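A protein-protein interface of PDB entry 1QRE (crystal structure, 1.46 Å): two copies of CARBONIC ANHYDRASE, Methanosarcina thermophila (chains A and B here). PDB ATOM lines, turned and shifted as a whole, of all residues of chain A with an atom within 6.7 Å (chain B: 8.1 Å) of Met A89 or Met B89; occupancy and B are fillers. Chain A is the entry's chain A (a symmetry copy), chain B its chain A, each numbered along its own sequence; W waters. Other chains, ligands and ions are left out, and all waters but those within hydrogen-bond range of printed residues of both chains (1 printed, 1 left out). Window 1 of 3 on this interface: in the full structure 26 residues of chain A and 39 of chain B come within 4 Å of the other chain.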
ATOM      1  N   ASP A  69       1.457  21.567 -31.373  1.00  0.00           N
ATOM      2  CA  ASP A  69       0.894  22.899 -31.572  1.00  0.00           C
ATOM      3  C   ASP A  69       1.993  23.878 -31.897  1.00  0.00           C
ATOM      4  O   ASP A  69       3.117  23.861 -31.383  1.00  0.00           O
ATOM      5  CB  ASP A  69       0.148  23.304 -30.288  1.00  0.00           C
ATOM      6  CG  ASP A  69      -0.657  24.562 -30.518  1.00  0.00           C
ATOM      7  OD1 ASP A  69      -1.842  24.369 -30.926  1.00  0.00           O
ATOM      8  OD2 ASP A  69      -0.160  25.673 -30.304  1.00  0.00           O
ATOM      9  N   GLN A  71       2.344  26.771 -30.896  1.00  0.00           N
ATOM     10  CA  GLN A  71       2.720  27.484 -29.688  1.00  0.00           C
ATOM     11  C   GLN A  71       3.227  26.570 -28.562  1.00  0.00           C
ATOM     12  O   GLN A  71       3.378  27.027 -27.407  1.00  0.00           O
ATOM     13  CB  GLN A  71       1.576  28.387 -29.213  1.00  0.00           C
ATOM     14  CG  GLN A  71       1.390  29.562 -30.192  1.00  0.00           C
ATOM     15  CD  GLN A  71       0.206  30.467 -29.895  1.00  0.00           C
ATOM     16  OE1 GLN A  71      -0.923  30.072 -30.240  1.00  0.00           O
ATOM     17  NE2 GLN A  71       0.343  31.588 -29.402  1.00  0.00           N
ATOM     18  N   ALA A  72       3.601  25.351 -28.890  1.00  0.00           N
ATOM     19  CA  ALA A  72       4.354  24.474 -28.003  1.00  0.00           C
ATOM     20  C   ALA A  72       5.808  24.577 -28.374  1.00  0.00           C
ATOM     21  O   ALA A  72       6.156  25.055 -29.491  1.00  0.00           O
ATOM     22  CB  ALA A  72       3.861  23.039 -28.091  1.00  0.00           C
ATOM     23  N   SER A  73       6.729  24.183 -27.519  1.00  0.00           N
ATOM     24  CA  SER A  73       8.150  24.163 -27.769  1.00  0.00           C
ATOM     25  C   SER A  73       8.710  22.790 -27.548  1.00  0.00           C
ATOM     26  O   SER A  73       8.411  22.223 -26.460  1.00  0.00           O
ATOM     27  CB  SER A  73       8.862  25.163 -26.866  1.00  0.00           C
ATOM     28  OG  SER A  73      10.278  25.124 -26.976  1.00  0.00           O
ATOM     29  N   SER A  87      -0.035  20.272 -26.721  1.00  0.00           N
ATOM     30  CA  SER A  87      -0.897  21.458 -26.739  1.00  0.00           C
ATOM     31  C   SER A  87      -0.187  22.780 -26.603  1.00  0.00           C
ATOM     32  O   SER A  87       1.008  22.873 -26.306  1.00  0.00           O
ATOM     33  CB  SER A  87      -1.836  21.337 -25.514  1.00  0.00           C
ATOM     34  OG  SER A  87      -2.766  20.260 -25.651  1.00  0.00           O
ATOM     35  N   PRO A  88      -0.897  23.894 -26.799  1.00  0.00           N
ATOM     36  CA  PRO A  88      -0.323  25.221 -26.676  1.00  0.00           C
ATOM     37  C   PRO A  88       0.419  25.369 -25.366  1.00  0.00           C
ATOM     38  O   PRO A  88      -0.088  24.975 -24.312  1.00  0.00           O
ATOM     39  CB  PRO A  88      -1.483  26.215 -26.772  1.00  0.00           C
ATOM     40  CG  PRO A  88      -2.469  25.445 -27.620  1.00  0.00           C
ATOM     41  CD  PRO A  88      -2.330  23.986 -27.167  1.00  0.00           C
ATOM     42  N   MET A  89       1.559  26.064 -25.404  1.00  0.00           N
ATOM     43  CA  MET A  89       2.306  26.482 -24.235  1.00  0.00           C
ATOM     44  C   MET A  89       3.003  25.356 -23.488  1.00  0.00           C
ATOM     45  O   MET A  89       3.667  25.615 -22.464  1.00  0.00           O
ATOM     46  CB  MET A  89       1.465  27.326 -23.288  1.00  0.00           C
ATOM     47  CG  MET A  89       0.575  28.393 -23.867  1.00  0.00           C
ATOM     48  SD  MET A  89       1.447  29.517 -24.994  1.00  0.00           S
ATOM     49  CE  MET A  89       0.049  30.243 -25.850  1.00  0.00           C
ATOM     50  N   ALA A  90       2.945  24.137 -23.980  1.00  0.00           N
ATOM     51  CA  ALA A  90       3.781  23.085 -23.417  1.00  0.00           C
ATOM     52  C   ALA A  90       5.220  23.300 -23.783  1.00  0.00           C
ATOM     53  O   ALA A  90       5.514  23.784 -24.893  1.00  0.00           O
ATOM     54  CB  ALA A  90       3.327  21.719 -23.956  1.00  0.00           C
ATOM     55  N   SER A  91       6.123  22.900 -22.916  1.00  0.00           N
ATOM     56  CA  SER A  91       7.543  23.003 -23.173  1.00  0.00           C
ATOM     57  C   SER A  91       8.221  21.700 -22.860  1.00  0.00           C
ATOM     58  O   SER A  91       8.227  21.277 -21.680  1.00  0.00           O
ATOM     59  CB  SER A  91       8.173  24.155 -22.397  1.00  0.00           C
ATOM     60  OG  SER A  91       9.563  24.251 -22.746  1.00  0.00           O
ATOM     61  N   GLN A 109      -0.504  18.280 -22.286  1.00  0.00           N
ATOM     62  CA  GLN A 109      -1.481  19.356 -22.338  1.00  0.00           C
ATOM     63  C   GLN A 109      -0.893  20.741 -22.085  1.00  0.00           C
ATOM     64  O   GLN A 109       0.321  20.939 -21.971  1.00  0.00           O
ATOM     65  CB  GLN A 109      -2.696  19.015 -21.463  1.00  0.00           C
ATOM     66  CG  GLN A 109      -3.331  17.675 -21.899  1.00  0.00           C
ATOM     67  CD  GLN A 109      -4.535  17.393 -21.019  1.00  0.00           C
ATOM     68  OE1 GLN A 109      -5.142  18.201 -20.337  1.00  0.00           O
ATOM     69  NE2 GLN A 109      -4.877  16.094 -21.050  1.00  0.00           N
ATOM     70  N   ASP A 110      -1.810  21.723 -22.101  1.00  0.00           N
ATOM     71  CA  ASP A 110      -1.383  23.130 -22.175  1.00  0.00           C
ATOM     72  C   ASP A 110      -0.535  23.493 -20.995  1.00  0.00           C
ATOM     73  O   ASP A 110      -0.852  23.203 -19.827  1.00  0.00           O
ATOM     74  CB  ASP A 110      -2.555  24.134 -22.242  1.00  0.00           C
ATOM     75  CG  ASP A 110      -3.718  23.680 -23.088  1.00  0.00           C
ATOM     76  OD1 ASP A 110      -4.300  22.601 -22.835  1.00  0.00           O
ATOM     77  OD2 ASP A 110      -4.003  24.371 -24.107  1.00  0.00           O
ATOM     78  N   GLY A 111       0.616  24.110 -21.242  1.00  0.00           N
ATOM     79  CA  GLY A 111       1.492  24.588 -20.194  1.00  0.00           C
ATOM     80  C   GLY A 111       2.213  23.483 -19.492  1.00  0.00           C
ATOM     81  O   GLY A 111       2.884  23.790 -18.455  1.00  0.00           O
ATOM     82  N   VAL A 112       2.175  22.230 -19.916  1.00  0.00           N
ATOM     83  CA  VAL A 112       2.959  21.198 -19.271  1.00  0.00           C
ATOM     84  C   VAL A 112       4.449  21.359 -19.527  1.00  0.00           C
ATOM     85  O   VAL A 112       4.826  21.695 -20.676  1.00  0.00           O
ATOM     86  CB  VAL A 112       2.478  19.821 -19.740  1.00  0.00           C
ATOM     87  CG1 VAL A 112       3.424  18.693 -19.305  1.00  0.00           C
ATOM     88  CG2 VAL A 112       1.105  19.516 -19.148  1.00  0.00           C
ATOM     89  N   VAL A 113       5.307  21.109 -18.533  1.00  0.00           N
ATOM     90  CA  VAL A 113       6.740  21.173 -18.758  1.00  0.00           C
ATOM     91  C   VAL A 113       7.351  19.795 -18.510  1.00  0.00           C
ATOM     92  O   VAL A 113       7.056  19.162 -17.481  1.00  0.00           O
ATOM     93  CB  VAL A 113       7.398  22.219 -17.815  1.00  0.00           C
ATOM     94  CG1 VAL A 113       8.949  22.208 -17.869  1.00  0.00           C
ATOM     95  CG2 VAL A 113       6.900  23.609 -18.132  1.00  0.00           C
ATOM     96  N   PHE B  42       1.988  30.742 -37.747  1.00  0.00           N
ATOM     97  CA  PHE B  42       0.666  30.316 -37.309  1.00  0.00           C
ATOM     98  C   PHE B  42      -0.271  31.452 -36.924  1.00  0.00           C
ATOM     99  O   PHE B  42       0.169  32.591 -36.739  1.00  0.00           O
ATOM    100  CB  PHE B  42       0.886  29.464 -36.026  1.00  0.00           C
ATOM    101  CG  PHE B  42       1.577  30.242 -34.935  1.00  0.00           C
ATOM    102  CD1 PHE B  42       0.846  30.921 -33.985  1.00  0.00           C
ATOM    103  CD2 PHE B  42       2.959  30.301 -34.858  1.00  0.00           C
ATOM    104  CE1 PHE B  42       1.469  31.658 -32.989  1.00  0.00           C
ATOM    105  CE2 PHE B  42       3.598  31.022 -33.863  1.00  0.00           C
ATOM    106  CZ  PHE B  42       2.848  31.700 -32.918  1.00  0.00           C
ATOM    107  N   ASN B  44      -2.727  32.618 -33.850  1.00  0.00           N
ATOM    108  CA  ASN B  44      -2.971  32.279 -32.439  1.00  0.00           C
ATOM    109  C   ASN B  44      -4.440  32.310 -32.109  1.00  0.00           C
ATOM    110  O   ASN B  44      -4.824  31.876 -31.000  1.00  0.00           O
ATOM    111  CB  ASN B  44      -2.197  33.225 -31.532  1.00  0.00           C
ATOM    112  CG  ASN B  44      -2.668  34.662 -31.611  1.00  0.00           C
ATOM    113  OD1 ASN B  44      -2.984  35.138 -32.709  1.00  0.00           O
ATOM    114  ND2 ASN B  44      -2.760  35.327 -30.490  1.00  0.00           N
ATOM    115  N   ASP B  69      -3.108  38.978 -26.330  1.00  0.00           N
ATOM    116  CA  ASP B  69      -1.671  39.036 -26.571  1.00  0.00           C
ATOM    117  C   ASP B  69      -1.298  38.101 -27.691  1.00  0.00           C
ATOM    118  O   ASP B  69      -1.809  36.989 -27.870  1.00  0.00           O
ATOM    119  CB  ASP B  69      -0.947  38.661 -25.265  1.00  0.00           C
ATOM    120  CG  ASP B  69       0.534  38.939 -25.381  1.00  0.00           C
ATOM    121  OD1 ASP B  69       0.887  40.103 -25.027  1.00  0.00           O
ATOM    122  OD2 ASP B  69       1.306  38.066 -25.790  1.00  0.00           O
ATOM    123  N   PRO B  70      -0.309  38.498 -28.501  1.00  0.00           N
ATOM    124  CA  PRO B  70       0.159  37.656 -29.598  1.00  0.00           C
ATOM    125  C   PRO B  70       0.705  36.301 -29.174  1.00  0.00           C
ATOM    126  O   PRO B  70       0.668  35.323 -29.924  1.00  0.00           O
ATOM    127  CB  PRO B  70       1.251  38.493 -30.306  1.00  0.00           C
ATOM    128  CG  PRO B  70       1.623  39.504 -29.236  1.00  0.00           C
ATOM    129  CD  PRO B  70       0.317  39.828 -28.495  1.00  0.00           C
ATOM    130  N   GLN B  71       1.148  36.236 -27.903  1.00  0.00           N
ATOM    131  CA  GLN B  71       1.639  34.993 -27.339  1.00  0.00           C
ATOM    132  C   GLN B  71       0.619  34.271 -26.447  1.00  0.00           C
ATOM    133  O   GLN B  71       0.982  33.308 -25.734  1.00  0.00           O
ATOM    134  CB  GLN B  71       2.969  35.215 -26.611  1.00  0.00           C
ATOM    135  CG  GLN B  71       4.082  35.526 -27.631  1.00  0.00           C
ATOM    136  CD  GLN B  71       5.430  35.884 -27.025  1.00  0.00           C
ATOM    137  OE1 GLN B  71       5.578  37.040 -26.592  1.00  0.00           O
ATOM    138  NE2 GLN B  71       6.378  35.098 -27.023  1.00  0.00           N
ATOM    139  N   ALA B  72      -0.645  34.623 -26.558  1.00  0.00           N
ATOM    140  CA  ALA B  72      -1.749  33.853 -25.998  1.00  0.00           C
ATOM    141  C   ALA B  72      -2.320  32.995 -27.093  1.00  0.00           C
ATOM    142  O   ALA B  72      -2.072  33.250 -28.307  1.00  0.00           O
ATOM    143  CB  ALA B  72      -2.810  34.762 -25.399  1.00  0.00           C
ATOM    144  N   SER B  73      -3.068  31.957 -26.785  1.00  0.00           N
ATOM    145  CA  SER B  73      -3.731  31.091 -27.731  1.00  0.00           C
ATOM    146  C   SER B  73      -5.204  31.036 -27.459  1.00  0.00           C
ATOM    147  O   SER B  73      -5.553  30.795 -26.269  1.00  0.00           O
ATOM    148  CB  SER B  73      -3.140  29.689 -27.671  1.00  0.00           C
ATOM    149  OG  SER B  73      -3.815  28.750 -28.497  1.00  0.00           O
ATOM    150  N   VAL B  74      -6.115  31.228 -28.403  1.00  0.00           N
ATOM    151  CA  VAL B  74      -7.542  31.191 -28.227  1.00  0.00           C
ATOM    152  C   VAL B  74      -8.106  30.358 -29.379  1.00  0.00           C
ATOM    153  O   VAL B  74      -7.983  30.726 -30.552  1.00  0.00           O
ATOM    154  CB  VAL B  74      -8.206  32.588 -28.239  1.00  0.00           C
ATOM    155  CG1 VAL B  74      -9.687  32.466 -27.951  1.00  0.00           C
ATOM    156  CG2 VAL B  74      -7.528  33.512 -27.243  1.00  0.00           C
ATOM    157  N   VAL B  86      -6.240  39.362 -22.305  1.00  0.00           N
ATOM    158  CA  VAL B  86      -5.739  37.995 -22.328  1.00  0.00           C
ATOM    159  C   VAL B  86      -4.235  38.128 -22.449  1.00  0.00           C
ATOM    160  O   VAL B  86      -3.726  38.614 -23.483  1.00  0.00           O
ATOM    161  CB  VAL B  86      -6.353  37.113 -23.377  1.00  0.00           C
ATOM    162  CG1 VAL B  86      -5.797  35.688 -23.259  1.00  0.00           C
ATOM    163  CG2 VAL B  86      -7.885  37.058 -23.250  1.00  0.00           C
ATOM    164  N   SER B  87      -3.497  37.708 -21.451  1.00  0.00           N
ATOM    165  CA  SER B  87      -2.050  37.924 -21.349  1.00  0.00           C
ATOM    166  C   SER B  87      -1.187  36.870 -21.994  1.00  0.00           C
ATOM    167  O   SER B  87      -1.636  35.801 -22.414  1.00  0.00           O
ATOM    168  CB  SER B  87      -1.711  37.906 -19.838  1.00  0.00           C
ATOM    169  OG  SER B  87      -2.255  39.034 -19.149  1.00  0.00           O
ATOM    170  N   PRO B  88       0.122  37.111 -22.092  1.00  0.00           N
ATOM    171  CA  PRO B  88       1.051  36.161 -22.677  1.00  0.00           C
ATOM    172  C   PRO B  88       0.877  34.788 -22.065  1.00  0.00           C
ATOM    173  O   PRO B  88       0.774  34.657 -20.841  1.00  0.00           O
ATOM    174  CB  PRO B  88       2.459  36.706 -22.423  1.00  0.00           C
ATOM    175  CG  PRO B  88       2.198  38.194 -22.359  1.00  0.00           C
ATOM    176  CD  PRO B  88       0.843  38.330 -21.655  1.00  0.00           C
ATOM    177  N   MET B  89       0.983  33.750 -22.895  1.00  0.00           N
ATOM    178  CA  MET B  89       1.044  32.364 -22.476  1.00  0.00           C
ATOM    179  C   MET B  89      -0.260  31.806 -21.927  1.00  0.00           C
ATOM    180  O   MET B  89      -0.307  30.623 -21.534  1.00  0.00           O
ATOM    181  CB  MET B  89       2.195  32.105 -21.515  1.00  0.00           C
ATOM    182  CG  MET B  89       3.536  32.720 -21.811  1.00  0.00           C
ATOM    183  SD  MET B  89       4.124  32.379 -23.494  1.00  0.00           S
ATOM    184  CE  MET B  89       5.384  33.645 -23.647  1.00  0.00           C
ATOM    185  N   ALA B  90      -1.332  32.569 -21.941  1.00  0.00           N
ATOM    186  CA  ALA B  90      -2.637  31.997 -21.633  1.00  0.00           C
ATOM    187  C   ALA B  90      -3.100  31.106 -22.749  1.00  0.00           C
ATOM    188  O   ALA B  90      -2.823  31.393 -23.929  1.00  0.00           O
ATOM    189  CB  ALA B  90      -3.662  33.123 -21.435  1.00  0.00           C
ATOM    190  N   SER B  91      -3.845  30.076 -22.419  1.00  0.00           N
ATOM    191  CA  SER B  91      -4.398  29.172 -23.406  1.00  0.00           C
ATOM    192  C   SER B  91      -5.861  28.951 -23.143  1.00  0.00           C
ATOM    193  O   SER B  91      -6.216  28.386 -22.081  1.00  0.00           O
ATOM    194  CB  SER B  91      -3.637  27.852 -23.448  1.00  0.00           C
ATOM    195  OG  SER B  91      -4.185  27.027 -24.489  1.00  0.00           O
ATOM    196  N   ILE B  92      -6.740  29.438 -23.998  1.00  0.00           N
ATOM    197  CA  ILE B  92      -8.184  29.268 -23.914  1.00  0.00           C
ATOM    198  C   ILE B  92      -8.539  28.297 -25.030  1.00  0.00           C
ATOM    199  O   ILE B  92      -8.375  28.645 -26.207  1.00  0.00           O
ATOM    200  CB  ILE B  92      -8.919  30.605 -24.083  1.00  0.00           C
ATOM    201  CG1 ILE B  92      -8.473  31.606 -23.028  1.00  0.00           C
ATOM    202  CG2 ILE B  92     -10.424  30.324 -23.982  1.00  0.00           C
ATOM    203  CD1 ILE B  92      -9.066  33.009 -23.199  1.00  0.00           C
ATOM    204  N   VAL B 108      -7.667  37.383 -18.121  1.00  0.00           N
ATOM    205  CA  VAL B 108      -7.124  35.997 -18.200  1.00  0.00           C
ATOM    206  C   VAL B 108      -5.616  36.175 -18.223  1.00  0.00           C
ATOM    207  O   VAL B 108      -5.072  36.548 -19.276  1.00  0.00           O
ATOM    208  CB  VAL B 108      -7.645  35.296 -19.453  1.00  0.00           C
ATOM    209  CG1 VAL B 108      -7.105  33.872 -19.531  1.00  0.00           C
ATOM    210  CG2 VAL B 108      -9.175  35.249 -19.487  1.00  0.00           C
ATOM    211  N   GLN B 109      -4.972  36.076 -17.091  1.00  0.00           N
ATOM    212  CA  GLN B 109      -3.573  36.434 -16.923  1.00  0.00           C
ATOM    213  C   GLN B 109      -2.597  35.376 -17.426  1.00  0.00           C
ATOM    214  O   GLN B 109      -2.964  34.366 -18.034  1.00  0.00           O
ATOM    215  CB  GLN B 109      -3.312  36.902 -15.484  1.00  0.00           C
ATOM    216  CG  GLN B 109      -4.232  38.088 -15.114  1.00  0.00           C
ATOM    217  CD  GLN B 109      -3.923  38.523 -13.692  1.00  0.00           C
ATOM    218  OE1 GLN B 109      -2.914  38.268 -13.058  1.00  0.00           O
ATOM    219  NE2 GLN B 109      -4.929  39.242 -13.166  1.00  0.00           N
ATOM    220  N   ASP B 110      -1.307  35.702 -17.235  1.00  0.00           N
ATOM    221  CA  ASP B 110      -0.245  34.949 -17.921  1.00  0.00           C
ATOM    222  C   ASP B 110      -0.279  33.504 -17.531  1.00  0.00           C
ATOM    223  O   ASP B 110      -0.371  33.131 -16.346  1.00  0.00           O
ATOM    224  CB  ASP B 110       1.177  35.482 -17.641  1.00  0.00           C
ATOM    225  CG  ASP B 110       1.278  36.985 -17.572  1.00  0.00           C
ATOM    226  OD1 ASP B 110       0.582  37.627 -16.756  1.00  0.00           O
ATOM    227  OD2 ASP B 110       2.002  37.562 -18.433  1.00  0.00           O
ATOM    228  N   GLY B 111      -0.251  32.610 -18.513  1.00  0.00           N
ATOM    229  CA  GLY B 111      -0.197  31.182 -18.276  1.00  0.00           C
ATOM    230  C   GLY B 111      -1.494  30.627 -17.780  1.00  0.00           C
ATOM    231  O   GLY B 111      -1.501  29.415 -17.395  1.00  0.00           O
ATOM    232  N   VAL B 112      -2.604  31.347 -17.742  1.00  0.00           N
ATOM    233  CA  VAL B 112      -3.864  30.756 -17.347  1.00  0.00           C
ATOM    234  C   VAL B 112      -4.397  29.781 -18.386  1.00  0.00           C
ATOM    235  O   VAL B 112      -4.290  30.083 -19.599  1.00  0.00           O
ATOM    236  CB  VAL B 112      -4.887  31.863 -17.073  1.00  0.00           C
ATOM    237  CG1 VAL B 112      -6.310  31.316 -16.905  1.00  0.00           C
ATOM    238  CG2 VAL B 112      -4.529  32.602 -15.787  1.00  0.00           C
ATOM    239  N   VAL B 113      -4.986  28.654 -17.975  1.00  0.00           N
ATOM    240  CA  VAL B 113      -5.579  27.737 -18.930  1.00  0.00           C
ATOM    241  C   VAL B 113      -7.078  27.628 -18.662  1.00  0.00           C
ATOM    242  O   VAL B 113      -7.490  27.443 -17.503  1.00  0.00           O
ATOM    243  CB  VAL B 113      -4.922  26.331 -18.824  1.00  0.00           C
ATOM    244  CG1 VAL B 113      -5.632  25.252 -19.683  1.00  0.00           C
ATOM    245  CG2 VAL B 113      -3.463  26.395 -19.210  1.00  0.00           C
ATOM    246  N   GLN B 152      -1.211  31.965 -13.845  1.00  0.00           N
ATOM    247  CA  GLN B 152      -0.993  30.542 -13.690  1.00  0.00           C
ATOM    248  C   GLN B 152      -2.172  29.831 -13.047  1.00  0.00           C
ATOM    249  O   GLN B 152      -2.068  28.623 -12.785  1.00  0.00           O
ATOM    250  CB  GLN B 152       0.293  30.221 -12.932  1.00  0.00           C
ATOM    251  CG  GLN B 152       1.545  30.764 -13.597  1.00  0.00           C
ATOM    252  CD  GLN B 152       2.777  30.498 -12.778  1.00  0.00           C
ATOM    253  OE1 GLN B 152       2.730  30.448 -11.535  1.00  0.00           O
ATOM    254  NE2 GLN B 152       3.940  30.323 -13.375  1.00  0.00           N
HETATM  255  O   HOH W   1       2.640  31.863 -27.518  1.00  0.00           O
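O of Ala B72 lies within hydrogen-bond range of NE2 of Gln A71, at 3.1 Å. OG of Ser B91 sits at hydrogen-bond distance from OD2 of Asp A110 (2.7 Å).
The backbone carbonyl oxygen of Asn B44 lies within hydrogen-bond range of the backbone NH of Val B74. O of Ser B73 sits at hydrogen-bond distance from N of Ile B92 (2.9 Å). ND2 of Asn B44 sits at hydrogen-bond distance from O of Pro B70 (3.5 Å). O of Ala B90 lies within hydrogen-bond range of N of Ser B73, 2.9 Å away. The backbone carbonyl oxygen (O) of Pro A88 is in hydrogen-bond range of the backbone NH (N) of Gly A111, at 3.3 Å. The side-chain carboxylate (OD2) of Asp B69 is in hydrogen-bond range of the backbone NH (N) of Gln B71 (2.8 Å).
Among the printed residues, pairs that only touch across the chains: Gln A71 with Phe B42 (3.5 Å), Gln A71 with Asn B44 (3.6 Å), Gln A71 with Pro B70 (3.8 Å), Gln A71 with Ser B73 (3.4 Å), Pro A88 with Ser B73 (3.7 Å), Pro A88 with Ser B91 (3.6 Å), Met A89 with Gln B71 (3.2 Å), Met A89 with Ala B72 (3.8 Å), Met A89 with Ser B73 (3.7 Å), Met A89 with Met B89 (3.3 Å), Met A89 with Ala B90 (3.6 Å) and Asp A110 with Val B113 (3.9 Å).
Ala A72 touches none of the printed residues of chain B. Met A89 touches five residues of chain B. No residue of chain B comes within 4 Å of Ala A90. Val A113 touches none of the printed residues of chain B. Printed residues of chain A within 4 Å of Ala B72: Gln A71 (3.1 Å) and Met A89 (3.8 Å). Met B89 touches just one residue of chain A: Met A89. Printed residues of chain A within 4 Å of Ser B91: Pro A88 and Asp A110. Printed residues of chain A within 4 Å of Val B113: Asp A110. The nearest residue of chain B that does not touch Met A89 is Ser B91 (4.3 Å).
Printed residues of chain B that touch a printed residue of chain A: Phe B42, Asn B44, Pro B70, Gln B71, Ala B72, Ser B73, Met B89, Ala B90, Ser B91 and Val B113. Hydrophobic or aromatic side chains of chain B that line the printed part of chain A: Phe B42 and Val B113. Among the printed residues, no Asp or Glu carboxylate lies within 4 Å of a Lys or Arg side-chain nitrogen of the other chain.
Gln A71 touches Ala B72, but with the chains exchanged Ala A72 does not touch Gln B71 (9.0 Å). Pro A88 touches Ser B91, but with the chains exchanged Ser A91 does not touch Pro B88 (12.9 Å). Met A89 touches Ala B72, but with the chains exchanged Ala A72 does not touch Met B89 (8.9 Å). Met A89 touches Ser B73, but with the chains exchanged Ser A73 does not touch Met B89 (9.3 Å). Of the 14 pairs that touch across the chains among the printed residues, 1 has its exchanged pair printed and touching as well.
Water W1 lies within hydrogen-bond range of O of Gln B71, NE2 of Gln A71 and SD of Met A89.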
